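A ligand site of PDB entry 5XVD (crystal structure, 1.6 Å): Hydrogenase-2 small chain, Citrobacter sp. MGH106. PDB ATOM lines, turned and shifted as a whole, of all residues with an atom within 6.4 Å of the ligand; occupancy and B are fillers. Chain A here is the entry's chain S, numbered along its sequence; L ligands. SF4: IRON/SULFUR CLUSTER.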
ATOM      1  N   ILE A 191     -15.989  19.498  26.222  1.00  0.00           N
ATOM      2  CA  ILE A 191     -14.872  18.543  26.298  1.00  0.00           C
ATOM      3  C   ILE A 191     -15.324  17.136  25.907  1.00  0.00           C
ATOM      4  O   ILE A 191     -14.624  16.426  25.184  1.00  0.00           O
ATOM      5  CB  ILE A 191     -14.226  18.572  27.714  1.00  0.00           C
ATOM      6  CG1 ILE A 191     -13.470  19.906  27.901  1.00  0.00           C
ATOM      7  CG2 ILE A 191     -13.282  17.391  27.938  1.00  0.00           C
ATOM      8  CD1 ILE A 191     -13.120  20.233  29.334  1.00  0.00           C
ATOM      9  N   HIS A 192     -16.525  16.763  26.342  1.00  0.00           N
ATOM     10  CA  HIS A 192     -17.115  15.447  26.072  1.00  0.00           C
ATOM     11  C   HIS A 192     -17.392  15.245  24.575  1.00  0.00           C
ATOM     12  O   HIS A 192     -17.470  14.104  24.101  1.00  0.00           O
ATOM     13  CB  HIS A 192     -18.405  15.317  26.885  1.00  0.00           C
ATOM     14  CG  HIS A 192     -19.150  14.024  26.712  1.00  0.00           C
ATOM     15  ND1 HIS A 192     -18.715  12.831  27.245  1.00  0.00           N
ATOM     16  CD2 HIS A 192     -20.335  13.746  26.116  1.00  0.00           C
ATOM     17  CE1 HIS A 192     -19.570  11.875  26.972  1.00  0.00           C
ATOM     18  NE2 HIS A 192     -20.567  12.400  26.285  1.00  0.00           N
ATOM     19  N   GLU A 193     -17.527  16.352  23.846  1.00  0.00           N
ATOM     20  CA  GLU A 193     -17.795  16.287  22.410  1.00  0.00           C
ATOM     21  C   GLU A 193     -16.508  16.289  21.586  1.00  0.00           C
ATOM     22  O   GLU A 193     -16.546  16.410  20.359  1.00  0.00           O
ATOM     23  CB  GLU A 193     -18.740  17.409  21.999  1.00  0.00           C
ATOM     24  CG  GLU A 193     -20.137  17.255  22.617  1.00  0.00           C
ATOM     25  CD  GLU A 193     -20.809  15.953  22.201  1.00  0.00           C
ATOM     26  OE1 GLU A 193     -20.895  15.682  20.986  1.00  0.00           O
ATOM     27  OE2 GLU A 193     -21.256  15.189  23.088  1.00  0.00           O
ATOM     28  N   CYS A 195     -13.650  14.184  23.184  1.00  0.00           N
ATOM     29  CA  CYS A 195     -12.861  13.397  24.126  1.00  0.00           C
ATOM     30  C   CYS A 195     -12.528  12.000  23.602  1.00  0.00           C
ATOM     31  O   CYS A 195     -13.412  11.271  23.124  1.00  0.00           O
ATOM     32  CB  CYS A 195     -13.593  13.261  25.457  1.00  0.00           C
ATOM     33  SG  CYS A 195     -12.649  12.292  26.657  1.00  0.00           S
ATOM     34  N   GLU A 196     -11.266  11.639  23.718  1.00  0.00           N
ATOM     35  CA  GLU A 196     -10.796  10.345  23.205  1.00  0.00           C
ATOM     36  C   GLU A 196     -11.335   9.144  23.970  1.00  0.00           C
ATOM     37  O   GLU A 196     -11.182   8.014  23.516  1.00  0.00           O
ATOM     38  CB  GLU A 196      -9.269  10.327  23.166  1.00  0.00           C
ATOM     39  CG  GLU A 196      -8.611  10.299  24.537  1.00  0.00           C
ATOM     40  CD  GLU A 196      -8.321  11.668  25.138  1.00  0.00           C
ATOM     41  OE1 GLU A 196      -8.977  12.671  24.742  1.00  0.00           O
ATOM     42  OE2 GLU A 196      -7.424  11.716  26.007  1.00  0.00           O
ATOM     43  N   ARG A 197     -11.949   9.358  25.137  1.00  0.00           N
ATOM     44  CA  ARG A 197     -12.563   8.237  25.856  1.00  0.00           C
ATOM     45  C   ARG A 197     -14.037   8.031  25.527  1.00  0.00           C
ATOM     46  O   ARG A 197     -14.671   7.141  26.069  1.00  0.00           O
ATOM     47  CB  ARG A 197     -12.364   8.339  27.367  1.00  0.00           C
ATOM     48  CG  ARG A 197     -10.880   8.492  27.701  1.00  0.00           C
ATOM     49  CD  ARG A 197     -10.544   8.190  29.147  1.00  0.00           C
ATOM     50  NE  ARG A 197      -9.100   8.233  29.331  1.00  0.00           N
ATOM     51  CZ  ARG A 197      -8.461   7.740  30.378  1.00  0.00           C
ATOM     52  NH1 ARG A 197      -9.146   7.148  31.355  1.00  0.00           N
ATOM     53  NH2 ARG A 197      -7.137   7.822  30.448  1.00  0.00           N
ATOM     54  N   ARG A 198     -14.560   8.867  24.634  1.00  0.00           N
ATOM     55  CA  ARG A 198     -15.941   8.716  24.196  1.00  0.00           C
ATOM     56  C   ARG A 198     -16.311   7.308  23.696  1.00  0.00           C
ATOM     57  O   ARG A 198     -17.412   6.830  23.990  1.00  0.00           O
ATOM     58  CB  ARG A 198     -16.279   9.779  23.133  1.00  0.00           C
ATOM     59  CG  ARG A 198     -17.702   9.712  22.664  1.00  0.00           C
ATOM     60  CD  ARG A 198     -18.736   9.990  23.770  1.00  0.00           C
ATOM     61  NE  ARG A 198     -20.061  10.026  23.159  1.00  0.00           N
ATOM     62  CZ  ARG A 198     -20.663  11.149  22.750  1.00  0.00           C
ATOM     63  NH1 ARG A 198     -20.078  12.323  22.953  1.00  0.00           N
ATOM     64  NH2 ARG A 198     -21.853  11.085  22.174  1.00  0.00           N
ATOM     65  N   PRO A 199     -15.407   6.611  22.966  1.00  0.00           N
ATOM     66  CA  PRO A 199     -15.771   5.234  22.580  1.00  0.00           C
ATOM     67  C   PRO A 199     -16.083   4.339  23.783  1.00  0.00           C
ATOM     68  O   PRO A 199     -16.944   3.454  23.697  1.00  0.00           O
ATOM     69  CB  PRO A 199     -14.505   4.731  21.871  1.00  0.00           C
ATOM     70  CG  PRO A 199     -13.828   5.965  21.364  1.00  0.00           C
ATOM     71  CD  PRO A 199     -14.102   7.022  22.401  1.00  0.00           C
ATOM     72  N   PHE A 201     -17.265   5.443  26.792  1.00  0.00           N
ATOM     73  CA  PHE A 201     -18.566   5.937  27.234  1.00  0.00           C
ATOM     74  C   PHE A 201     -19.676   5.256  26.418  1.00  0.00           C
ATOM     75  O   PHE A 201     -20.658   4.765  26.970  1.00  0.00           O
ATOM     76  CB  PHE A 201     -18.611   7.459  27.065  1.00  0.00           C
ATOM     77  CG  PHE A 201     -19.940   8.067  27.390  1.00  0.00           C
ATOM     78  CD1 PHE A 201     -20.917   8.216  26.409  1.00  0.00           C
ATOM     79  CD2 PHE A 201     -20.231   8.522  28.672  1.00  0.00           C
ATOM     80  CE1 PHE A 201     -22.134   8.779  26.700  1.00  0.00           C
ATOM     81  CE2 PHE A 201     -21.456   9.097  28.964  1.00  0.00           C
ATOM     82  CZ  PHE A 201     -22.405   9.222  27.975  1.00  0.00           C
ATOM     83  N   PHE A 206     -16.702   1.729  31.809  1.00  0.00           N
ATOM     84  CA  PHE A 206     -16.516   2.805  32.781  1.00  0.00           C
ATOM     85  C   PHE A 206     -15.580   2.388  33.897  1.00  0.00           C
ATOM     86  O   PHE A 206     -15.700   1.287  34.445  1.00  0.00           O
ATOM     87  CB  PHE A 206     -17.860   3.203  33.412  1.00  0.00           C
ATOM     88  CG  PHE A 206     -18.833   3.815  32.465  1.00  0.00           C
ATOM     89  CD1 PHE A 206     -18.555   5.019  31.844  1.00  0.00           C
ATOM     90  CD2 PHE A 206     -20.056   3.195  32.200  1.00  0.00           C
ATOM     91  CE1 PHE A 206     -19.471   5.580  30.964  1.00  0.00           C
ATOM     92  CE2 PHE A 206     -20.963   3.760  31.334  1.00  0.00           C
ATOM     93  CZ  PHE A 206     -20.677   4.953  30.713  1.00  0.00           C
ATOM     94  N   TRP A 219     -10.387   3.560  30.557  1.00  0.00           N
ATOM     95  CA  TRP A 219     -11.816   3.674  30.241  1.00  0.00           C
ATOM     96  C   TRP A 219     -12.376   5.034  30.645  1.00  0.00           C
ATOM     97  O   TRP A 219     -11.700   5.851  31.281  1.00  0.00           O
ATOM     98  CB  TRP A 219     -12.601   2.540  30.903  1.00  0.00           C
ATOM     99  CG  TRP A 219     -12.341   1.201  30.298  1.00  0.00           C
ATOM    100  CD1 TRP A 219     -11.460   0.905  29.296  1.00  0.00           C
ATOM    101  CD2 TRP A 219     -12.974  -0.031  30.661  1.00  0.00           C
ATOM    102  NE1 TRP A 219     -11.504  -0.450  29.020  1.00  0.00           N
ATOM    103  CE2 TRP A 219     -12.428  -1.044  29.843  1.00  0.00           C
ATOM    104  CE3 TRP A 219     -13.955  -0.382  31.606  1.00  0.00           C
ATOM    105  CZ2 TRP A 219     -12.834  -2.379  29.933  1.00  0.00           C
ATOM    106  CZ3 TRP A 219     -14.345  -1.706  31.696  1.00  0.00           C
ATOM    107  CH2 TRP A 219     -13.781  -2.690  30.864  1.00  0.00           C
ATOM    108  N   CYS A 220     -13.629   5.280  30.271  1.00  0.00           N
ATOM    109  CA  CYS A 220     -14.277   6.567  30.499  1.00  0.00           C
ATOM    110  C   CYS A 220     -14.460   6.822  31.992  1.00  0.00           C
ATOM    111  O   CYS A 220     -14.707   5.889  32.767  1.00  0.00           O
ATOM    112  CB  CYS A 220     -15.624   6.597  29.761  1.00  0.00           C
ATOM    113  SG  CYS A 220     -16.747   7.913  30.254  1.00  0.00           S
ATOM    114  N   LEU A 221     -14.371   8.091  32.384  1.00  0.00           N
ATOM    115  CA  LEU A 221     -14.370   8.482  33.804  1.00  0.00           C
ATOM    116  C   LEU A 221     -15.696   9.109  34.264  1.00  0.00           C
ATOM    117  O   LEU A 221     -15.751   9.692  35.343  1.00  0.00           O
ATOM    118  CB  LEU A 221     -13.203   9.451  34.094  1.00  0.00           C
ATOM    119  CG  LEU A 221     -11.816   8.935  33.685  1.00  0.00           C
ATOM    120  CD1 LEU A 221     -10.709   9.945  34.063  1.00  0.00           C
ATOM    121  CD2 LEU A 221     -11.500   7.539  34.251  1.00  0.00           C
ATOM    122  N   TYR A 222     -16.735   8.969  33.454  1.00  0.00           N
ATOM    123  CA  TYR A 222     -18.053   9.542  33.756  1.00  0.00           C
ATOM    124  C   TYR A 222     -18.521   9.217  35.172  1.00  0.00           C
ATOM    125  O   TYR A 222     -18.941  10.103  35.933  1.00  0.00           O
ATOM    126  CB  TYR A 222     -19.120   9.049  32.760  1.00  0.00           C
ATOM    127  CG  TYR A 222     -20.476   9.715  32.918  1.00  0.00           C
ATOM    128  CD1 TYR A 222     -21.423   9.253  33.830  1.00  0.00           C
ATOM    129  CD2 TYR A 222     -20.813  10.821  32.146  1.00  0.00           C
ATOM    130  CE1 TYR A 222     -22.663   9.885  33.961  1.00  0.00           C
ATOM    131  CE2 TYR A 222     -22.038  11.447  32.263  1.00  0.00           C
ATOM    132  CZ  TYR A 222     -22.960  10.984  33.174  1.00  0.00           C
ATOM    133  OH  TYR A 222     -24.185  11.610  33.291  1.00  0.00           O
ATOM    134  N   HIS A 223     -18.452   7.943  35.538  1.00  0.00           N
ATOM    135  CA  HIS A 223     -18.954   7.519  36.839  1.00  0.00           C
ATOM    136  C   HIS A 223     -18.002   7.805  37.996  1.00  0.00           C
ATOM    137  O   HIS A 223     -18.314   7.508  39.152  1.00  0.00           O
ATOM    138  CB  HIS A 223     -19.415   6.080  36.794  1.00  0.00           C
ATOM    139  CG  HIS A 223     -20.686   5.915  36.041  1.00  0.00           C
ATOM    140  ND1 HIS A 223     -21.925   6.183  36.594  1.00  0.00           N
ATOM    141  CD2 HIS A 223     -20.921   5.596  34.738  1.00  0.00           C
ATOM    142  CE1 HIS A 223     -22.859   5.987  35.687  1.00  0.00           C
ATOM    143  NE2 HIS A 223     -22.287   5.635  34.553  1.00  0.00           N
ATOM    144  N   CYS A 226     -16.840  12.769  36.075  1.00  0.00           N
ATOM    145  CA  CYS A 226     -16.313  13.626  35.004  1.00  0.00           C
ATOM    146  C   CYS A 226     -17.307  14.694  34.559  1.00  0.00           C
ATOM    147  O   CYS A 226     -18.459  14.391  34.215  1.00  0.00           O
ATOM    148  CB  CYS A 226     -15.891  12.780  33.805  1.00  0.00           C
ATOM    149  SG  CYS A 226     -14.996  13.761  32.570  1.00  0.00           S
ATOM    150  N   LYS A 227     -16.857  15.944  34.556  1.00  0.00           N
ATOM    151  CA  LYS A 227     -17.709  17.049  34.149  1.00  0.00           C
ATOM    152  C   LYS A 227     -17.504  17.453  32.695  1.00  0.00           C
ATOM    153  O   LYS A 227     -18.042  18.474  32.260  1.00  0.00           O
ATOM    154  CB  LYS A 227     -17.473  18.252  35.059  1.00  0.00           C
ATOM    155  CG  LYS A 227     -17.582  17.941  36.540  1.00  0.00           C
ATOM    156  CD  LYS A 227     -18.934  17.318  36.882  1.00  0.00           C
ATOM    157  CE  LYS A 227     -19.160  17.268  38.389  1.00  0.00           C
ATOM    158  NZ  LYS A 227     -18.061  16.546  39.116  1.00  0.00           N
ATOM    159  N   GLY A 228     -16.753  16.659  31.939  1.00  0.00           N
ATOM    160  CA  GLY A 228     -16.629  16.892  30.511  1.00  0.00           C
ATOM    161  C   GLY A 228     -17.946  17.117  29.771  1.00  0.00           C
ATOM    162  O   GLY A 228     -18.010  17.958  28.876  1.00  0.00           O
ATOM    163  N   PRO A 229     -19.006  16.352  30.105  1.00  0.00           N
ATOM    164  CA  PRO A 229     -20.292  16.549  29.441  1.00  0.00           C
ATOM    165  C   PRO A 229     -20.950  17.925  29.622  1.00  0.00           C
ATOM    166  O   PRO A 229     -21.881  18.252  28.877  1.00  0.00           O
ATOM    167  CB  PRO A 229     -21.175  15.456  30.064  1.00  0.00           C
ATOM    168  CG  PRO A 229     -20.209  14.354  30.333  1.00  0.00           C
ATOM    169  CD  PRO A 229     -18.959  15.047  30.811  1.00  0.00           C
ATOM    170  N   TRP A 247      -3.512  15.815  30.067  1.00  0.00           N
ATOM    171  CA  TRP A 247      -4.659  16.553  30.580  1.00  0.00           C
ATOM    172  C   TRP A 247      -5.250  15.704  31.696  1.00  0.00           C
ATOM    173  O   TRP A 247      -4.872  14.554  31.842  1.00  0.00           O
ATOM    174  CB  TRP A 247      -5.660  16.961  29.494  1.00  0.00           C
ATOM    175  CG  TRP A 247      -6.489  15.898  28.828  1.00  0.00           C
ATOM    176  CD1 TRP A 247      -6.045  14.914  27.993  1.00  0.00           C
ATOM    177  CD2 TRP A 247      -7.913  15.772  28.882  1.00  0.00           C
ATOM    178  NE1 TRP A 247      -7.109  14.153  27.549  1.00  0.00           N
ATOM    179  CE2 TRP A 247      -8.266  14.683  28.071  1.00  0.00           C
ATOM    180  CE3 TRP A 247      -8.930  16.477  29.538  1.00  0.00           C
ATOM    181  CZ2 TRP A 247      -9.594  14.269  27.894  1.00  0.00           C
ATOM    182  CZ3 TRP A 247     -10.253  16.074  29.368  1.00  0.00           C
ATOM    183  CH2 TRP A 247     -10.565  14.977  28.556  1.00  0.00           C
ATOM    184  N   VAL A 249      -8.004  14.015  32.389  1.00  0.00           N
ATOM    185  CA  VAL A 249      -8.599  12.723  32.070  1.00  0.00           C
ATOM    186  C   VAL A 249      -7.554  11.717  31.581  1.00  0.00           C
ATOM    187  O   VAL A 249      -7.568  10.557  31.968  1.00  0.00           O
ATOM    188  CB  VAL A 249      -9.769  12.878  31.061  1.00  0.00           C
ATOM    189  CG1 VAL A 249     -10.152  11.543  30.429  1.00  0.00           C
ATOM    190  CG2 VAL A 249     -10.964  13.527  31.743  1.00  0.00           C
ATOM    191  N   PRO A 254     -11.112  12.495  36.625  1.00  0.00           N
ATOM    192  CA  PRO A 254     -12.205  13.170  35.910  1.00  0.00           C
ATOM    193  C   PRO A 254     -12.004  14.679  35.775  1.00  0.00           C
ATOM    194  O   PRO A 254     -11.366  15.301  36.626  1.00  0.00           O
ATOM    195  CB  PRO A 254     -13.434  12.892  36.788  1.00  0.00           C
ATOM    196  CG  PRO A 254     -12.879  12.539  38.146  1.00  0.00           C
ATOM    197  CD  PRO A 254     -11.597  11.800  37.833  1.00  0.00           C
ATOM    198  N   CYS A 255     -12.542  15.254  34.712  1.00  0.00           N
ATOM    199  CA  CYS A 255     -12.669  16.702  34.629  1.00  0.00           C
ATOM    200  C   CYS A 255     -13.528  17.172  35.790  1.00  0.00           C
ATOM    201  O   CYS A 255     -14.521  16.525  36.133  1.00  0.00           O
ATOM    202  CB  CYS A 255     -13.304  17.087  33.289  1.00  0.00           C
ATOM    203  SG  CYS A 255     -13.772  18.826  33.126  1.00  0.00           S
HETATM  204 FE1  SF4 L   1     -15.942  10.019  29.505  1.00  0.00          FE
HETATM  205 FE2  SF4 L   1     -14.364  11.789  28.211  1.00  0.00          FE
HETATM  206 FE3  SF4 L   1     -16.970  12.262  28.435  1.00  0.00          FE
HETATM  207 FE4  SF4 L   1     -15.342  12.500  30.593  1.00  0.00          FE
HETATM  208  S1  SF4 L   1     -15.337  13.709  28.765  1.00  0.00           S
HETATM  209  S2  SF4 L   1     -17.308  11.486  30.457  1.00  0.00           S
HETATM  210  S3  SF4 L   1     -13.974  10.818  30.124  1.00  0.00           S
HETATM  211  S4  SF4 L   1     -16.001  10.557  27.385  1.00  0.00           S
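A ring nitrogen (ND1) of His 192 is bound to an iron atom (FE3) of the ligand, at 2.2 Å. SG of Cys 195 binds FE2 of the ligand (2.4 Å). An iron atom (FE4) of the ligand is bound by the side-chain sulfur of Cys 226 (2.4 Å). An iron atom (FE1) of the ligand is bound by the side-chain sulfur (SG) of Cys 220, at 2.4 Å. The backbone NH (N) of Arg 198 sits close to a sulfur (S4) of the ligand (3.5 Å). A sulfur (S3) of the ligand lies close to the backbone NH (N) of Leu 221.
NH1 of Arg 198 sits at hydrogen-bond distance from O of His 192, 3.4 Å away. The backbone carbonyl oxygen of Gly 228 lies within hydrogen-bond range of the backbone NH of His 192, at 3.2 Å. The backbone NH (N) of Cys 226 sits at hydrogen-bond distance from the backbone carbonyl oxygen (O) of Leu 221 (3.3 Å). The side-chain sulfur (SG) of Cys 226 lies close to the backbone NH (N) of Gly 228 (3.4 Å). The side-chain sulfur (SG) of Cys 226 sits close to the backbone NH (N) of Cys 255 (3.6 Å). The backbone NH (N) of Tyr 222 lies close to the side-chain sulfur (SG) of Cys 220 (3.4 Å). The guanidinium group (NH1) of Arg 198 is in salt-bridge range of the side-chain carboxylate (OE2) of Glu 193, 3.1 Å away. The guanidinium group (NH2) of Arg 197 is in hydrogen-bond range of the backbone carbonyl oxygen (O) of Val 249 (3.2 Å).
Residues that only touch the ligand: Arg 197 (3.7 Å), Tyr 222 (3.8 Å), Gly 228 (3.9 Å), Val 249 (3.9 Å) and Pro 229 (3.9 Å). Hydrophobic or aromatic side chains within 4 Å of the ligand: His 192, Tyr 222, Pro 229 and Val 249.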
